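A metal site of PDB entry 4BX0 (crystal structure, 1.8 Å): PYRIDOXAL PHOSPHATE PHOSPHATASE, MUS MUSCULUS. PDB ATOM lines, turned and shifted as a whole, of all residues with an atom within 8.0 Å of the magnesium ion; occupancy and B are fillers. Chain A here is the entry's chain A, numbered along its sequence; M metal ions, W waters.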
ATOM      1  N   PHE A  24     -24.319  -7.848  -8.087  1.00  0.00           N
ATOM      2  CA  PHE A  24     -23.532  -6.626  -8.227  1.00  0.00           C
ATOM      3  C   PHE A  24     -24.402  -5.456  -8.648  1.00  0.00           C
ATOM      4  O   PHE A  24     -25.123  -5.554  -9.643  1.00  0.00           O
ATOM      5  CB  PHE A  24     -22.474  -6.763  -9.314  1.00  0.00           C
ATOM      6  CG  PHE A  24     -21.394  -7.776  -9.034  1.00  0.00           C
ATOM      7  CD1 PHE A  24     -20.237  -7.411  -8.358  1.00  0.00           C
ATOM      8  CD2 PHE A  24     -21.510  -9.074  -9.488  1.00  0.00           C
ATOM      9  CE1 PHE A  24     -19.243  -8.322  -8.121  1.00  0.00           C
ATOM     10  CE2 PHE A  24     -20.517  -9.995  -9.253  1.00  0.00           C
ATOM     11  CZ  PHE A  24     -19.378  -9.630  -8.568  1.00  0.00           C
ATOM     12  N   ASP A  25     -24.310  -4.355  -7.913  1.00  0.00           N
ATOM     13  CA  ASP A  25     -24.658  -3.068  -8.471  1.00  0.00           C
ATOM     14  C   ASP A  25     -23.612  -2.779  -9.562  1.00  0.00           C
ATOM     15  O   ASP A  25     -22.544  -3.371  -9.567  1.00  0.00           O
ATOM     16  CB  ASP A  25     -24.597  -1.992  -7.379  1.00  0.00           C
ATOM     17  CG  ASP A  25     -24.728  -0.590  -7.920  1.00  0.00           C
ATOM     18  OD1 ASP A  25     -25.698  -0.310  -8.670  1.00  0.00           O
ATOM     19  OD2 ASP A  25     -23.848   0.223  -7.600  1.00  0.00           O
ATOM     20  N   CYS A  26     -23.934  -1.881 -10.485  1.00  0.00           N
ATOM     21  CA  CYS A  26     -23.072  -1.613 -11.639  1.00  0.00           C
ATOM     22  C   CYS A  26     -22.276  -0.304 -11.524  1.00  0.00           C
ATOM     23  O   CYS A  26     -21.051  -0.321 -11.432  1.00  0.00           O
ATOM     24  CB  CYS A  26     -23.897  -1.626 -12.927  1.00  0.00           C
ATOM     25  SG  CYS A  26     -24.770  -3.202 -13.205  1.00  0.00           S
ATOM     26  N   ASP A  27     -22.972   0.835 -11.551  1.00  0.00           N
ATOM     27  CA  ASP A  27     -22.275   2.126 -11.482  1.00  0.00           C
ATOM     28  C   ASP A  27     -21.555   2.269 -10.135  1.00  0.00           C
ATOM     29  O   ASP A  27     -22.164   2.129  -9.079  1.00  0.00           O
ATOM     30  CB  ASP A  27     -23.253   3.278 -11.710  1.00  0.00           C
ATOM     31  CG  ASP A  27     -23.862   3.264 -13.101  1.00  0.00           C
ATOM     32  OD1 ASP A  27     -23.118   3.427 -14.083  1.00  0.00           O
ATOM     33  OD2 ASP A  27     -25.098   3.104 -13.217  1.00  0.00           O
ATOM     34  N   GLY A  28     -20.247   2.509 -10.197  1.00  0.00           N
ATOM     35  CA  GLY A  28     -19.424   2.656  -9.008  1.00  0.00           C
ATOM     36  C   GLY A  28     -18.788   1.353  -8.543  1.00  0.00           C
ATOM     37  O   GLY A  28     -17.982   1.353  -7.604  1.00  0.00           O
ATOM     38  N   VAL A  29     -19.160   0.249  -9.192  1.00  0.00           N
ATOM     39  CA  VAL A  29     -18.694  -1.073  -8.807  1.00  0.00           C
ATOM     40  C   VAL A  29     -17.957  -1.760  -9.943  1.00  0.00           C
ATOM     41  O   VAL A  29     -16.866  -2.296  -9.759  1.00  0.00           O
ATOM     42  CB  VAL A  29     -19.891  -1.979  -8.413  1.00  0.00           C
ATOM     43  CG1 VAL A  29     -19.429  -3.399  -8.130  1.00  0.00           C
ATOM     44  CG2 VAL A  29     -20.618  -1.404  -7.210  1.00  0.00           C
ATOM     45  N   LEU A  30     -18.577  -1.749 -11.123  1.00  0.00           N
ATOM     46  CA  LEU A  30     -17.973  -2.340 -12.305  1.00  0.00           C
ATOM     47  C   LEU A  30     -17.293  -1.263 -13.143  1.00  0.00           C
ATOM     48  O   LEU A  30     -16.378  -1.555 -13.898  1.00  0.00           O
ATOM     49  CB  LEU A  30     -19.046  -2.998 -13.178  1.00  0.00           C
ATOM     50  CG  LEU A  30     -19.928  -4.077 -12.535  1.00  0.00           C
ATOM     51  CD1 LEU A  30     -20.866  -4.632 -13.568  1.00  0.00           C
ATOM     52  CD2 LEU A  30     -19.085  -5.181 -11.913  1.00  0.00           C
ATOM     53  N   TRP A  31     -17.781  -0.037 -13.009  1.00  0.00           N
ATOM     54  CA  TRP A  31     -17.324   1.071 -13.828  1.00  0.00           C
ATOM     55  C   TRP A  31     -17.796   2.401 -13.260  1.00  0.00           C
ATOM     56  O   TRP A  31     -18.723   2.466 -12.458  1.00  0.00           O
ATOM     57  CB  TRP A  31     -17.843   0.897 -15.264  1.00  0.00           C
ATOM     58  CG  TRP A  31     -19.340   0.856 -15.394  1.00  0.00           C
ATOM     59  CD1 TRP A  31     -20.220   1.837 -15.059  1.00  0.00           C
ATOM     60  CD2 TRP A  31     -20.127  -0.230 -15.913  1.00  0.00           C
ATOM     61  NE1 TRP A  31     -21.509   1.438 -15.333  1.00  0.00           N
ATOM     62  CE2 TRP A  31     -21.478   0.170 -15.851  1.00  0.00           C
ATOM     63  CE3 TRP A  31     -19.818  -1.499 -16.405  1.00  0.00           C
ATOM     64  CZ2 TRP A  31     -22.518  -0.650 -16.276  1.00  0.00           C
ATOM     65  CZ3 TRP A  31     -20.858  -2.318 -16.829  1.00  0.00           C
ATOM     66  CH2 TRP A  31     -22.194  -1.890 -16.759  1.00  0.00           C
ATOM     67  N   ASN A  32     -17.117   3.471 -13.653  1.00  0.00           N
ATOM     68  CA  ASN A  32     -17.567   4.839 -13.392  1.00  0.00           C
ATOM     69  C   ASN A  32     -17.530   5.604 -14.704  1.00  0.00           C
ATOM     70  O   ASN A  32     -16.454   5.858 -15.235  1.00  0.00           O
ATOM     71  CB  ASN A  32     -16.683   5.528 -12.357  1.00  0.00           C
ATOM     72  CG  ASN A  32     -16.874   4.973 -10.950  1.00  0.00           C
ATOM     73  OD1 ASN A  32     -17.913   5.187 -10.317  1.00  0.00           O
ATOM     74  ND2 ASN A  32     -15.878   4.242 -10.473  1.00  0.00           N
ATOM     75  N   VAL A  57     -27.806  -5.674 -10.770  1.00  0.00           N
ATOM     76  CA  VAL A  57     -28.945  -4.876 -10.376  1.00  0.00           C
ATOM     77  C   VAL A  57     -28.568  -3.424 -10.611  1.00  0.00           C
ATOM     78  O   VAL A  57     -27.436  -3.035 -10.343  1.00  0.00           O
ATOM     79  CB  VAL A  57     -29.314  -5.106  -8.900  1.00  0.00           C
ATOM     80  CG1 VAL A  57     -30.026  -6.426  -8.743  1.00  0.00           C
ATOM     81  CG2 VAL A  57     -28.083  -5.055  -8.019  1.00  0.00           C
ATOM     82  N   SER A  58     -29.482  -2.637 -11.173  1.00  0.00           N
ATOM     83  CA  SER A  58     -29.211  -1.223 -11.376  1.00  0.00           C
ATOM     84  C   SER A  58     -30.500  -0.429 -11.347  1.00  0.00           C
ATOM     85  O   SER A  58     -31.546  -0.919 -11.739  1.00  0.00           O
ATOM     86  CB  SER A  58     -28.487  -0.994 -12.705  1.00  0.00           C
ATOM     87  OG  SER A  58     -28.240   0.391 -12.913  1.00  0.00           O
ATOM     88  N   ASN A  59     -30.433   0.819 -10.878  1.00  0.00           N
ATOM     89  CA  ASN A  59     -31.584   1.716 -10.932  1.00  0.00           C
ATOM     90  C   ASN A  59     -31.536   2.603 -12.175  1.00  0.00           C
ATOM     91  O   ASN A  59     -32.447   3.396 -12.402  1.00  0.00           O
ATOM     92  CB  ASN A  59     -31.680   2.567  -9.657  1.00  0.00           C
ATOM     93  CG  ASN A  59     -32.166   1.763  -8.453  1.00  0.00           C
ATOM     94  OD1 ASN A  59     -32.778   0.709  -8.602  1.00  0.00           O
ATOM     95  ND2 ASN A  59     -31.881   2.257  -7.258  1.00  0.00           N
ATOM     96  N   ASP A 175     -33.160   7.324  -6.140  1.00  0.00           N
ATOM     97  CA  ASP A 175     -31.750   7.702  -6.149  1.00  0.00           C
ATOM     98  C   ASP A 175     -31.607   9.198  -6.224  1.00  0.00           C
ATOM     99  O   ASP A 175     -32.292   9.847  -7.004  1.00  0.00           O
ATOM    100  CB  ASP A 175     -31.038   7.107  -7.359  1.00  0.00           C
ATOM    101  CG  ASP A 175     -30.769   5.629  -7.230  1.00  0.00           C
ATOM    102  OD1 ASP A 175     -31.076   5.054  -6.163  1.00  0.00           O
ATOM    103  OD2 ASP A 175     -30.226   5.053  -8.190  1.00  0.00           O
ATOM    104  N   PRO A 179     -25.817   8.810 -12.929  1.00  0.00           N
ATOM    105  CA  PRO A 179     -24.501   8.982 -13.563  1.00  0.00           C
ATOM    106  C   PRO A 179     -24.583   9.104 -15.079  1.00  0.00           C
ATOM    107  O   PRO A 179     -25.306   8.334 -15.722  1.00  0.00           O
ATOM    108  CB  PRO A 179     -23.763   7.712 -13.163  1.00  0.00           C
ATOM    109  CG  PRO A 179     -24.813   6.694 -13.067  1.00  0.00           C
ATOM    110  CD  PRO A 179     -26.046   7.410 -12.542  1.00  0.00           C
ATOM    111  N   LYS A 209     -33.962  -0.663  -5.800  1.00  0.00           N
ATOM    112  CA  LYS A 209     -33.253  -0.732  -4.525  1.00  0.00           C
ATOM    113  C   LYS A 209     -33.229   0.652  -3.913  1.00  0.00           C
ATOM    114  O   LYS A 209     -33.114   1.648  -4.634  1.00  0.00           O
ATOM    115  CB  LYS A 209     -31.820  -1.284  -4.694  1.00  0.00           C
ATOM    116  CG  LYS A 209     -30.991  -0.693  -5.825  1.00  0.00           C
ATOM    117  CD  LYS A 209     -29.656  -1.428  -5.943  1.00  0.00           C
ATOM    118  CE  LYS A 209     -28.900  -1.038  -7.206  1.00  0.00           C
ATOM    119  NZ  LYS A 209     -28.195   0.274  -7.071  1.00  0.00           N
ATOM    120  N   VAL A 232     -23.044  -6.836  -3.513  1.00  0.00           N
ATOM    121  CA  VAL A 232     -21.868  -5.963  -3.646  1.00  0.00           C
ATOM    122  C   VAL A 232     -22.288  -4.617  -4.238  1.00  0.00           C
ATOM    123  O   VAL A 232     -22.827  -4.571  -5.340  1.00  0.00           O
ATOM    124  CB  VAL A 232     -20.810  -6.596  -4.567  1.00  0.00           C
ATOM    125  CG1 VAL A 232     -19.550  -5.716  -4.638  1.00  0.00           C
ATOM    126  CG2 VAL A 232     -20.459  -8.003  -4.097  1.00  0.00           C
ATOM    127  N   GLY A 233     -22.000  -3.537  -3.509  1.00  0.00           N
ATOM    128  CA  GLY A 233     -22.361  -2.211  -3.977  1.00  0.00           C
ATOM    129  C   GLY A 233     -21.427  -1.136  -3.450  1.00  0.00           C
ATOM    130  O   GLY A 233     -20.597  -1.392  -2.575  1.00  0.00           O
ATOM    131  N   ASP A 234     -21.575   0.074  -3.980  1.00  0.00           N
ATOM    132  CA  ASP A 234     -20.721   1.194  -3.600  1.00  0.00           C
ATOM    133  C   ASP A 234     -21.453   2.265  -2.784  1.00  0.00           C
ATOM    134  O   ASP A 234     -20.816   3.190  -2.277  1.00  0.00           O
ATOM    135  CB  ASP A 234     -20.141   1.854  -4.838  1.00  0.00           C
ATOM    136  CG  ASP A 234     -21.199   2.553  -5.658  1.00  0.00           C
ATOM    137  OD1 ASP A 234     -22.062   1.852  -6.225  1.00  0.00           O
ATOM    138  OD2 ASP A 234     -21.178   3.807  -5.758  1.00  0.00           O
ATOM    139  N   ARG A 235     -22.766   2.170  -2.664  1.00  0.00           N
ATOM    140  CA  ARG A 235     -23.511   3.165  -1.876  1.00  0.00           C
ATOM    141  C   ARG A 235     -24.236   2.530  -0.689  1.00  0.00           C
ATOM    142  O   ARG A 235     -24.960   1.554  -0.840  1.00  0.00           O
ATOM    143  CB  ARG A 235     -24.476   3.973  -2.735  1.00  0.00           C
ATOM    144  CG  ARG A 235     -25.164   5.085  -1.944  1.00  0.00           C
ATOM    145  CD  ARG A 235     -25.774   6.177  -2.823  1.00  0.00           C
ATOM    146  NE  ARG A 235     -26.200   7.322  -2.017  1.00  0.00           N
ATOM    147  CZ  ARG A 235     -27.438   7.513  -1.573  1.00  0.00           C
ATOM    148  NH1 ARG A 235     -28.408   6.649  -1.847  1.00  0.00           N
ATOM    149  NH2 ARG A 235     -27.711   8.586  -0.838  1.00  0.00           N
ATOM    150  N   THR A 238     -28.196   2.729  -0.396  1.00  0.00           N
ATOM    151  CA  THR A 238     -28.979   2.020  -1.403  1.00  0.00           C
ATOM    152  C   THR A 238     -28.632   0.520  -1.459  1.00  0.00           C
ATOM    153  O   THR A 238     -29.502  -0.327  -1.287  1.00  0.00           O
ATOM    154  CB  THR A 238     -28.731   2.622  -2.807  1.00  0.00           C
ATOM    155  OG1 THR A 238     -29.048   4.025  -2.803  1.00  0.00           O
ATOM    156  CG2 THR A 238     -29.580   1.913  -3.861  1.00  0.00           C
ATOM    157  N   ASP A 239     -27.361   0.208  -1.692  1.00  0.00           N
ATOM    158  CA  ASP A 239     -26.966  -1.169  -1.930  1.00  0.00           C
ATOM    159  C   ASP A 239     -26.817  -1.983  -0.645  1.00  0.00           C
ATOM    160  O   ASP A 239     -27.222  -3.147  -0.585  1.00  0.00           O
ATOM    161  CB  ASP A 239     -25.635  -1.214  -2.695  1.00  0.00           C
ATOM    162  CG  ASP A 239     -25.691  -0.425  -3.994  1.00  0.00           C
ATOM    163  OD1 ASP A 239     -26.604  -0.665  -4.809  1.00  0.00           O
ATOM    164  OD2 ASP A 239     -24.810   0.445  -4.190  1.00  0.00           O
ATOM    165  N   THR A 253     -17.758  -1.866  -1.773  1.00  0.00           N
ATOM    166  CA  THR A 253     -16.556  -1.617  -2.553  1.00  0.00           C
ATOM    167  C   THR A 253     -16.310  -0.117  -2.552  1.00  0.00           C
ATOM    168  O   THR A 253     -17.244   0.685  -2.521  1.00  0.00           O
ATOM    169  CB  THR A 253     -16.657  -2.191  -3.992  1.00  0.00           C
ATOM    170  OG1 THR A 253     -15.428  -1.985  -4.692  1.00  0.00           O
ATOM    171  CG2 THR A 253     -17.802  -1.565  -4.762  1.00  0.00           C
ATOM    172  N   GLY A 256     -16.555   3.694  -5.556  1.00  0.00           N
ATOM    173  CA  GLY A 256     -17.721   4.459  -5.903  1.00  0.00           C
ATOM    174  C   GLY A 256     -18.040   5.586  -4.937  1.00  0.00           C
ATOM    175  O   GLY A 256     -17.160   6.299  -4.477  1.00  0.00           O
ATOM    176  N   VAL A 257     -19.329   5.716  -4.625  1.00  0.00           N
ATOM    177  CA  VAL A 257     -19.846   6.879  -3.917  1.00  0.00           C
ATOM    178  C   VAL A 257     -19.469   6.945  -2.432  1.00  0.00           C
ATOM    179  O   VAL A 257     -19.061   7.998  -1.942  1.00  0.00           O
ATOM    180  CB  VAL A 257     -21.387   6.939  -4.023  1.00  0.00           C
ATOM    181  CG1 VAL A 257     -21.954   8.018  -3.116  1.00  0.00           C
ATOM    182  CG2 VAL A 257     -21.802   7.184  -5.474  1.00  0.00           C
ATOM    183  N   SER A 258     -19.607   5.822  -1.732  1.00  0.00           N
ATOM    184  CA  SER A 258     -19.444   5.824  -0.279  1.00  0.00           C
ATOM    185  C   SER A 258     -18.014   5.557   0.157  1.00  0.00           C
ATOM    186  O   SER A 258     -17.256   4.859  -0.511  1.00  0.00           O
ATOM    187  CB  SER A 258     -20.333   4.768   0.348  1.00  0.00           C
ATOM    188  OG  SER A 258     -21.708   5.100   0.243  1.00  0.00           O
HETATM  189 MG    MG M   1     -23.497   2.238  -7.566  1.00  0.00          MG
HETATM  190  O   HOH W   1     -24.837   2.346  -5.972  1.00  0.00           O
HETATM  191  O   HOH W   2     -23.055   4.275  -7.359  1.00  0.00           O
HETATM  192  O   HOH W   3     -24.991   2.554  -8.891  1.00  0.00           O
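Within 4 Å of the magnesium ion: Asp 25, Asp 27 and Asp 234.
The side-chain carboxylate of Asp 27 lies within hydrogen-bond range of the indole nitrogen of Trp 31 (2.8 Å).
O of Val 232 sits at hydrogen-bond distance from N of Asp 25 (3.0 Å).
N of Ser 258 lies within hydrogen-bond range of O of Asp 234.
OD1 of Asp 25 lies within salt-bridge range of NZ of Lys 209.
The backbone NH (N) of Val 257 lies within hydrogen-bond range of the side-chain carboxylate (OD2) of Asp 234.
N of Asp 234 lies within hydrogen-bond range of OD2 of Asp 239 (3.3 Å).
The magnesium ion is bound by OD1 of Asp 234 (2.0 Å), O of Asp 27 (2.0 Å), water W3 (2.0 Å), OD2 of Asp 25 (2.0 Å), water W1 (2.1 Å) and water W2 (2.1 Å).
The magnesium ion has six donor atoms within binding distance.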
